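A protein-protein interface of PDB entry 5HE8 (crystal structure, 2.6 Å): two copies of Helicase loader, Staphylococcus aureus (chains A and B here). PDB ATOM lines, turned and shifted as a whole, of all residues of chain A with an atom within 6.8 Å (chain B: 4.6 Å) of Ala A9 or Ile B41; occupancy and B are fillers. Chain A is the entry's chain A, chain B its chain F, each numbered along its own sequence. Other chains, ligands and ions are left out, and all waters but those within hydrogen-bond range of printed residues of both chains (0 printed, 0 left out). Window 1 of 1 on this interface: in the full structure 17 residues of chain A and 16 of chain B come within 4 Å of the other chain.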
ATOM      1  N   LEU A   6      -7.259   5.150 -20.694  1.00  0.00           N
ATOM      2  CA  LEU A   6      -7.635   6.472 -21.182  1.00  0.00           C
ATOM      3  C   LEU A   6      -7.861   7.434 -20.021  1.00  0.00           C
ATOM      4  O   LEU A   6      -8.155   7.012 -18.901  1.00  0.00           O
ATOM      5  CB  LEU A   6      -8.894   6.383 -22.049  1.00  0.00           C
ATOM      6  CG  LEU A   6      -8.798   5.480 -23.281  1.00  0.00           C
ATOM      7  CD1 LEU A   6     -10.143   5.394 -23.983  1.00  0.00           C
ATOM      8  CD2 LEU A   6      -7.724   5.970 -24.244  1.00  0.00           C
ATOM      9  N   ASP A   7      -7.726   8.730 -20.297  1.00  0.00           N
ATOM     10  CA  ASP A   7      -7.849   9.772 -19.279  1.00  0.00           C
ATOM     11  C   ASP A   7      -9.256  10.356 -19.352  1.00  0.00           C
ATOM     12  O   ASP A   7      -9.568  11.144 -20.249  1.00  0.00           O
ATOM     13  CB  ASP A   7      -6.792  10.852 -19.481  1.00  0.00           C
ATOM     14  CG  ASP A   7      -6.803  11.885 -18.374  1.00  0.00           C
ATOM     15  OD1 ASP A   7      -7.672  12.782 -18.408  1.00  0.00           O
ATOM     16  OD2 ASP A   7      -5.947  11.797 -17.471  1.00  0.00           O
ATOM     17  N   VAL A   8     -10.101   9.975 -18.392  1.00  0.00           N
ATOM     18  CA  VAL A   8     -11.470  10.476 -18.361  1.00  0.00           C
ATOM     19  C   VAL A   8     -11.514  11.902 -17.827  1.00  0.00           C
ATOM     20  O   VAL A   8     -12.383  12.688 -18.222  1.00  0.00           O
ATOM     21  CB  VAL A   8     -12.361   9.544 -17.521  1.00  0.00           C
ATOM     22  CG1 VAL A   8     -13.809  10.019 -17.542  1.00  0.00           C
ATOM     23  CG2 VAL A   8     -12.264   8.117 -18.027  1.00  0.00           C
ATOM     24  N   ALA A   9     -10.595  12.258 -16.928  1.00  0.00           N
ATOM     25  CA  ALA A   9     -10.595  13.602 -16.357  1.00  0.00           C
ATOM     26  C   ALA A   9     -10.505  14.662 -17.447  1.00  0.00           C
ATOM     27  O   ALA A   9     -11.282  15.625 -17.461  1.00  0.00           O
ATOM     28  CB  ALA A   9      -9.438  13.746 -15.369  1.00  0.00           C
ATOM     29  N   MET A  10      -9.561  14.501 -18.378  1.00  0.00           N
ATOM     30  CA  MET A  10      -9.388  15.509 -19.416  1.00  0.00           C
ATOM     31  C   MET A  10     -10.561  15.522 -20.387  1.00  0.00           C
ATOM     32  O   MET A  10     -10.923  16.585 -20.903  1.00  0.00           O
ATOM     33  CB  MET A  10      -8.082  15.279 -20.174  1.00  0.00           C
ATOM     34  CG  MET A  10      -7.635  16.497 -20.967  1.00  0.00           C
ATOM     35  SD  MET A  10      -7.308  17.922 -19.900  1.00  0.00           S
ATOM     36  CE  MET A  10      -7.555  19.279 -21.042  1.00  0.00           C
ATOM     37  N   ALA A  11     -11.163  14.361 -20.656  1.00  0.00           N
ATOM     38  CA  ALA A  11     -12.376  14.342 -21.463  1.00  0.00           C
ATOM     39  C   ALA A  11     -13.476  15.155 -20.797  1.00  0.00           C
ATOM     40  O   ALA A  11     -14.156  15.954 -21.454  1.00  0.00           O
ATOM     41  CB  ALA A  11     -12.832  12.902 -21.691  1.00  0.00           C
ATOM     42  N   ALA A  12     -13.653  14.977 -19.487  1.00  0.00           N
ATOM     43  CA  ALA A  12     -14.651  15.745 -18.751  1.00  0.00           C
ATOM     44  C   ALA A  12     -14.360  17.240 -18.829  1.00  0.00           C
ATOM     45  O   ALA A  12     -15.251  18.046 -19.125  1.00  0.00           O
ATOM     46  CB  ALA A  12     -14.692  15.277 -17.296  1.00  0.00           C
ATOM     47  N   ASP A  13     -13.114  17.630 -18.562  1.00  0.00           N
ATOM     48  CA  ASP A  13     -12.756  19.044 -18.618  1.00  0.00           C
ATOM     49  C   ASP A  13     -13.053  19.623 -19.997  1.00  0.00           C
ATOM     50  O   ASP A  13     -13.690  20.679 -20.122  1.00  0.00           O
ATOM     51  CB  ASP A  13     -11.278  19.216 -18.258  1.00  0.00           C
ATOM     52  CG  ASP A  13     -10.963  20.590 -17.697  1.00  0.00           C
ATOM     53  OD1 ASP A  13     -11.877  21.238 -17.144  1.00  0.00           O
ATOM     54  OD2 ASP A  13      -9.794  21.020 -17.800  1.00  0.00           O
ATOM     55  N   ASP A  14     -12.615  18.928 -21.050  1.00  0.00           N
ATOM     56  CA  ASP A  14     -12.773  19.444 -22.405  1.00  0.00           C
ATOM     57  C   ASP A  14     -14.242  19.532 -22.804  1.00  0.00           C
ATOM     58  O   ASP A  14     -14.646  20.480 -23.486  1.00  0.00           O
ATOM     59  CB  ASP A  14     -12.001  18.569 -23.393  1.00  0.00           C
ATOM     60  CG  ASP A  14     -10.496  18.735 -23.270  1.00  0.00           C
ATOM     61  OD1 ASP A  14     -10.040  19.864 -22.986  1.00  0.00           O
ATOM     62  OD2 ASP A  14      -9.768  17.737 -23.464  1.00  0.00           O
ATOM     63  N   PHE A  40     -18.799   9.979  -9.468  1.00  0.00           N
ATOM     64  CA  PHE A  40     -18.042  11.166  -9.082  1.00  0.00           C
ATOM     65  C   PHE A  40     -17.614  11.985 -10.293  1.00  0.00           C
ATOM     66  O   PHE A  40     -17.521  13.215 -10.200  1.00  0.00           O
ATOM     67  CB  PHE A  40     -16.813  10.773  -8.262  1.00  0.00           C
ATOM     68  CG  PHE A  40     -15.953  11.938  -7.877  1.00  0.00           C
ATOM     69  CD1 PHE A  40     -16.213  12.652  -6.722  1.00  0.00           C
ATOM     70  CD2 PHE A  40     -14.890  12.326  -8.675  1.00  0.00           C
ATOM     71  CE1 PHE A  40     -15.422  13.729  -6.365  1.00  0.00           C
ATOM     72  CE2 PHE A  40     -14.097  13.401  -8.323  1.00  0.00           C
ATOM     73  CZ  PHE A  40     -14.366  14.104  -7.167  1.00  0.00           C
ATOM     74  N   ILE A  41     -17.328  11.335 -11.423  1.00  0.00           N
ATOM     75  CA  ILE A  41     -16.970  12.081 -12.624  1.00  0.00           C
ATOM     76  C   ILE A  41     -18.195  12.782 -13.194  1.00  0.00           C
ATOM     77  O   ILE A  41     -18.115  13.936 -13.630  1.00  0.00           O
ATOM     78  CB  ILE A  41     -16.313  11.157 -13.666  1.00  0.00           C
ATOM     79  CG1 ILE A  41     -14.985  10.602 -13.143  1.00  0.00           C
ATOM     80  CG2 ILE A  41     -16.093  11.898 -14.985  1.00  0.00           C
ATOM     81  CD1 ILE A  41     -13.917  11.655 -12.898  1.00  0.00           C
ATOM     82  N   ALA A  44     -18.844  15.658 -11.001  1.00  0.00           N
ATOM     83  CA  ALA A  44     -17.795  16.652 -11.194  1.00  0.00           C
ATOM     84  C   ALA A  44     -18.044  17.467 -12.455  1.00  0.00           C
ATOM     85  O   ALA A  44     -17.847  18.688 -12.461  1.00  0.00           O
ATOM     86  CB  ALA A  44     -16.431  15.968 -11.260  1.00  0.00           C
ATOM     87  N   ALA B  12     -10.634  10.268  -5.058  1.00  0.00           N
ATOM     88  CA  ALA B  12     -11.222  11.577  -4.792  1.00  0.00           C
ATOM     89  C   ALA B  12     -12.577  11.436  -4.110  1.00  0.00           C
ATOM     90  O   ALA B  12     -12.865  12.122  -3.123  1.00  0.00           O
ATOM     91  CB  ALA B  12     -11.357  12.365  -6.094  1.00  0.00           C
ATOM     92  N   LEU B  30      -1.602  14.533  -7.463  1.00  0.00           N
ATOM     93  CA  LEU B  30      -1.904  14.238  -8.858  1.00  0.00           C
ATOM     94  C   LEU B  30      -0.783  14.775  -9.735  1.00  0.00           C
ATOM     95  O   LEU B  30      -0.581  15.991  -9.812  1.00  0.00           O
ATOM     96  CB  LEU B  30      -3.236  14.863  -9.263  1.00  0.00           C
ATOM     97  CG  LEU B  30      -4.402  14.629  -8.306  1.00  0.00           C
ATOM     98  CD1 LEU B  30      -5.637  15.379  -8.783  1.00  0.00           C
ATOM     99  CD2 LEU B  30      -4.689  13.146  -8.161  1.00  0.00           C
ATOM    100  N   THR B  36      -4.130  16.639 -18.715  1.00  0.00           N
ATOM    101  CA  THR B  36      -4.517  15.310 -18.265  1.00  0.00           C
ATOM    102  C   THR B  36      -5.616  15.341 -17.214  1.00  0.00           C
ATOM    103  O   THR B  36      -5.995  14.280 -16.708  1.00  0.00           O
ATOM    104  CB  THR B  36      -3.301  14.558 -17.703  1.00  0.00           C
ATOM    105  OG1 THR B  36      -2.605  15.388 -16.767  1.00  0.00           O
ATOM    106  CG2 THR B  36      -2.356  14.165 -18.815  1.00  0.00           C
ATOM    107  N   GLY B  37      -6.127  16.517 -16.864  1.00  0.00           N
ATOM    108  CA  GLY B  37      -7.261  16.625 -15.973  1.00  0.00           C
ATOM    109  C   GLY B  37      -6.933  16.785 -14.507  1.00  0.00           C
ATOM    110  O   GLY B  37      -7.829  16.617 -13.673  1.00  0.00           O
ATOM    111  N   LYS B  38      -5.685  17.110 -14.163  1.00  0.00           N
ATOM    112  CA  LYS B  38      -5.329  17.310 -12.761  1.00  0.00           C
ATOM    113  C   LYS B  38      -6.161  18.427 -12.140  1.00  0.00           C
ATOM    114  O   LYS B  38      -6.798  18.241 -11.092  1.00  0.00           O
ATOM    115  CB  LYS B  38      -3.836  17.623 -12.648  1.00  0.00           C
ATOM    116  CG  LYS B  38      -2.928  16.586 -13.295  1.00  0.00           C
ATOM    117  CD  LYS B  38      -1.460  16.825 -12.958  1.00  0.00           C
ATOM    118  CE  LYS B  38      -0.914  18.092 -13.608  1.00  0.00           C
ATOM    119  NZ  LYS B  38      -0.876  17.994 -15.094  1.00  0.00           N
ATOM    120  N   SER B  39      -6.169  19.601 -12.777  1.00  0.00           N
ATOM    121  CA  SER B  39      -6.938  20.725 -12.254  1.00  0.00           C
ATOM    122  C   SER B  39      -8.428  20.416 -12.215  1.00  0.00           C
ATOM    123  O   SER B  39      -9.146  20.946 -11.358  1.00  0.00           O
ATOM    124  CB  SER B  39      -6.679  21.974 -13.093  1.00  0.00           C
ATOM    125  OG  SER B  39      -5.333  22.401 -12.962  1.00  0.00           O
ATOM    126  N   PHE B  40      -8.915  19.571 -13.127  1.00  0.00           N
ATOM    127  CA  PHE B  40     -10.326  19.200 -13.099  1.00  0.00           C
ATOM    128  C   PHE B  40     -10.640  18.320 -11.896  1.00  0.00           C
ATOM    129  O   PHE B  40     -11.733  18.413 -11.325  1.00  0.00           O
ATOM    130  CB  PHE B  40     -10.721  18.486 -14.390  1.00  0.00           C
ATOM    131  CG  PHE B  40     -12.129  17.960 -14.375  1.00  0.00           C
ATOM    132  CD1 PHE B  40     -13.203  18.805 -14.610  1.00  0.00           C
ATOM    133  CD2 PHE B  40     -12.379  16.622 -14.116  1.00  0.00           C
ATOM    134  CE1 PHE B  40     -14.502  18.324 -14.591  1.00  0.00           C
ATOM    135  CE2 PHE B  40     -13.676  16.135 -14.098  1.00  0.00           C
ATOM    136  CZ  PHE B  40     -14.737  16.988 -14.335  1.00  0.00           C
ATOM    137  N   ILE B  41      -9.705  17.452 -11.502  1.00  0.00           N
ATOM    138  CA  ILE B  41      -9.925  16.609 -10.329  1.00  0.00           C
ATOM    139  C   ILE B  41      -9.852  17.444  -9.057  1.00  0.00           C
ATOM    140  O   ILE B  41     -10.675  17.289  -8.145  1.00  0.00           O
ATOM    141  CB  ILE B  41      -8.913  15.449 -10.296  1.00  0.00           C
ATOM    142  CG1 ILE B  41      -9.088  14.540 -11.517  1.00  0.00           C
ATOM    143  CG2 ILE B  41      -9.057  14.647  -9.004  1.00  0.00           C
ATOM    144  CD1 ILE B  41     -10.411  13.792 -11.570  1.00  0.00           C
ATOM    145  N   LEU B  42      -8.860  18.333  -8.964  1.00  0.00           N
ATOM    146  CA  LEU B  42      -8.790  19.214  -7.801  1.00  0.00           C
ATOM    147  C   LEU B  42     -10.054  20.060  -7.690  1.00  0.00           C
ATOM    148  O   LEU B  42     -10.636  20.194  -6.607  1.00  0.00           O
ATOM    149  CB  LEU B  42      -7.551  20.106  -7.877  1.00  0.00           C
ATOM    150  CG  LEU B  42      -6.179  19.433  -7.797  1.00  0.00           C
ATOM    151  CD1 LEU B  42      -5.098  20.492  -7.667  1.00  0.00           C
ATOM    152  CD2 LEU B  42      -6.094  18.447  -6.641  1.00  0.00           C
ATOM    153  N   GLY B  43     -10.499  20.634  -8.809  1.00  0.00           N
ATOM    154  CA  GLY B  43     -11.738  21.392  -8.796  1.00  0.00           C
ATOM    155  C   GLY B  43     -12.946  20.546  -8.450  1.00  0.00           C
ATOM    156  O   GLY B  43     -13.883  21.027  -7.812  1.00  0.00           O
ATOM    157  N   ALA B  44     -12.942  19.276  -8.862  1.00  0.00           N
ATOM    158  CA  ALA B  44     -14.046  18.382  -8.535  1.00  0.00           C
ATOM    159  C   ALA B  44     -14.108  18.110  -7.041  1.00  0.00           C
ATOM    160  O   ALA B  44     -15.196  18.072  -6.457  1.00  0.00           O
ATOM    161  CB  ALA B  44     -13.905  17.074  -9.312  1.00  0.00           C
ATOM    162  N   ILE B  45     -12.950  17.904  -6.406  1.00  0.00           N
ATOM    163  CA  ILE B  45     -12.920  17.744  -4.954  1.00  0.00           C
ATOM    164  C   ILE B  45     -13.379  19.026  -4.276  1.00  0.00           C
ATOM    165  O   ILE B  45     -14.166  18.997  -3.319  1.00  0.00           O
ATOM    166  CB  ILE B  45     -11.507  17.335  -4.492  1.00  0.00           C
ATOM    167  CG1 ILE B  45     -11.088  16.019  -5.155  1.00  0.00           C
ATOM    168  CG2 ILE B  45     -11.464  17.192  -2.977  1.00  0.00           C
ATOM    169  CD1 ILE B  45      -9.635  15.642  -4.925  1.00  0.00           C
ATOM    170  N   LEU B 166      -1.562  10.513 -13.925  1.00  0.00           N
ATOM    171  CA  LEU B 166      -2.573  10.784 -14.944  1.00  0.00           C
ATOM    172  C   LEU B 166      -1.865  10.924 -16.289  1.00  0.00           C
ATOM    173  O   LEU B 166      -1.229  11.948 -16.557  1.00  0.00           O
ATOM    174  CB  LEU B 166      -3.368  12.044 -14.605  1.00  0.00           C
ATOM    175  CG  LEU B 166      -4.541  11.909 -13.630  1.00  0.00           C
ATOM    176  CD1 LEU B 166      -4.086  11.446 -12.255  1.00  0.00           C
ATOM    177  CD2 LEU B 166      -5.285  13.232 -13.521  1.00  0.00           C
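OD1 of Asp A7 lies within hydrogen-bond range of N of Ala A9. OD1 of Asp A7 is in hydrogen-bond range of N of Met A10 (2.6 Å).
Ala A12 touches Phe B40, and with the chains exchanged Phe A40 touches Ala B12. Phe A40 touches Ala B44, and with the chains exchanged Ala A44 touches Phe B40. Ala B44 touches its own counterpart, Ala A44. Positions printed for both chains: 12, 40, 41 and 44.
Among the printed residues, no Asp or Glu carboxylate lies within 4 Å of a Lys or Arg side-chain nitrogen of the other chain.
O of Thr B36 sits close to OD2 of Asp A7 (2.6 Å). The backbone NH (N) of Thr B36 lies within hydrogen-bond range of the side-chain sulfur (SD) of Met A10 (3.6 Å). The side-chain sulfur of Met A10 sits at hydrogen-bond distance from the backbone NH of Gly B37 (3.5 Å).
Asp A7 touches Leu B166 (OD2 to CB, 3.9 Å). Thr B36 touches Ala A9. Ala A9 touches Phe B40 (O to CD2, 3.7 Å). Ala A9 touches Ile B41 (CB to CD1, 3.9 Å). Phe B40 touches Ala A12. Asp A13 touches Phe B40. CZ of Phe A40 touches CB of Ala B12, at 3.6 Å. Ala B44 touches Phe A40. Phe B40 touches Ala A44 (CZ to CB, 3.7 Å). Ala A44 touches Ala B44.
Leu A6 touches none of the printed residues of chain B. Printed residues of chain B within 4 Å of Asp A7: Thr B36 and Leu B166. Ala A9 touches just these residues of chain B: Thr B36 (3.7 Å), Gly B37 (3.7 Å), Phe B40 (3.7 Å) and Ile B41 (3.9 Å). Of the printed residues of chain B, Asp A13 touches Phe B40. Of chain A, only Ala A9 comes within 4 Å of Ile B41. The nearest printed residue of chain A that does not touch Thr B36 is Val A8 (6.1 Å).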
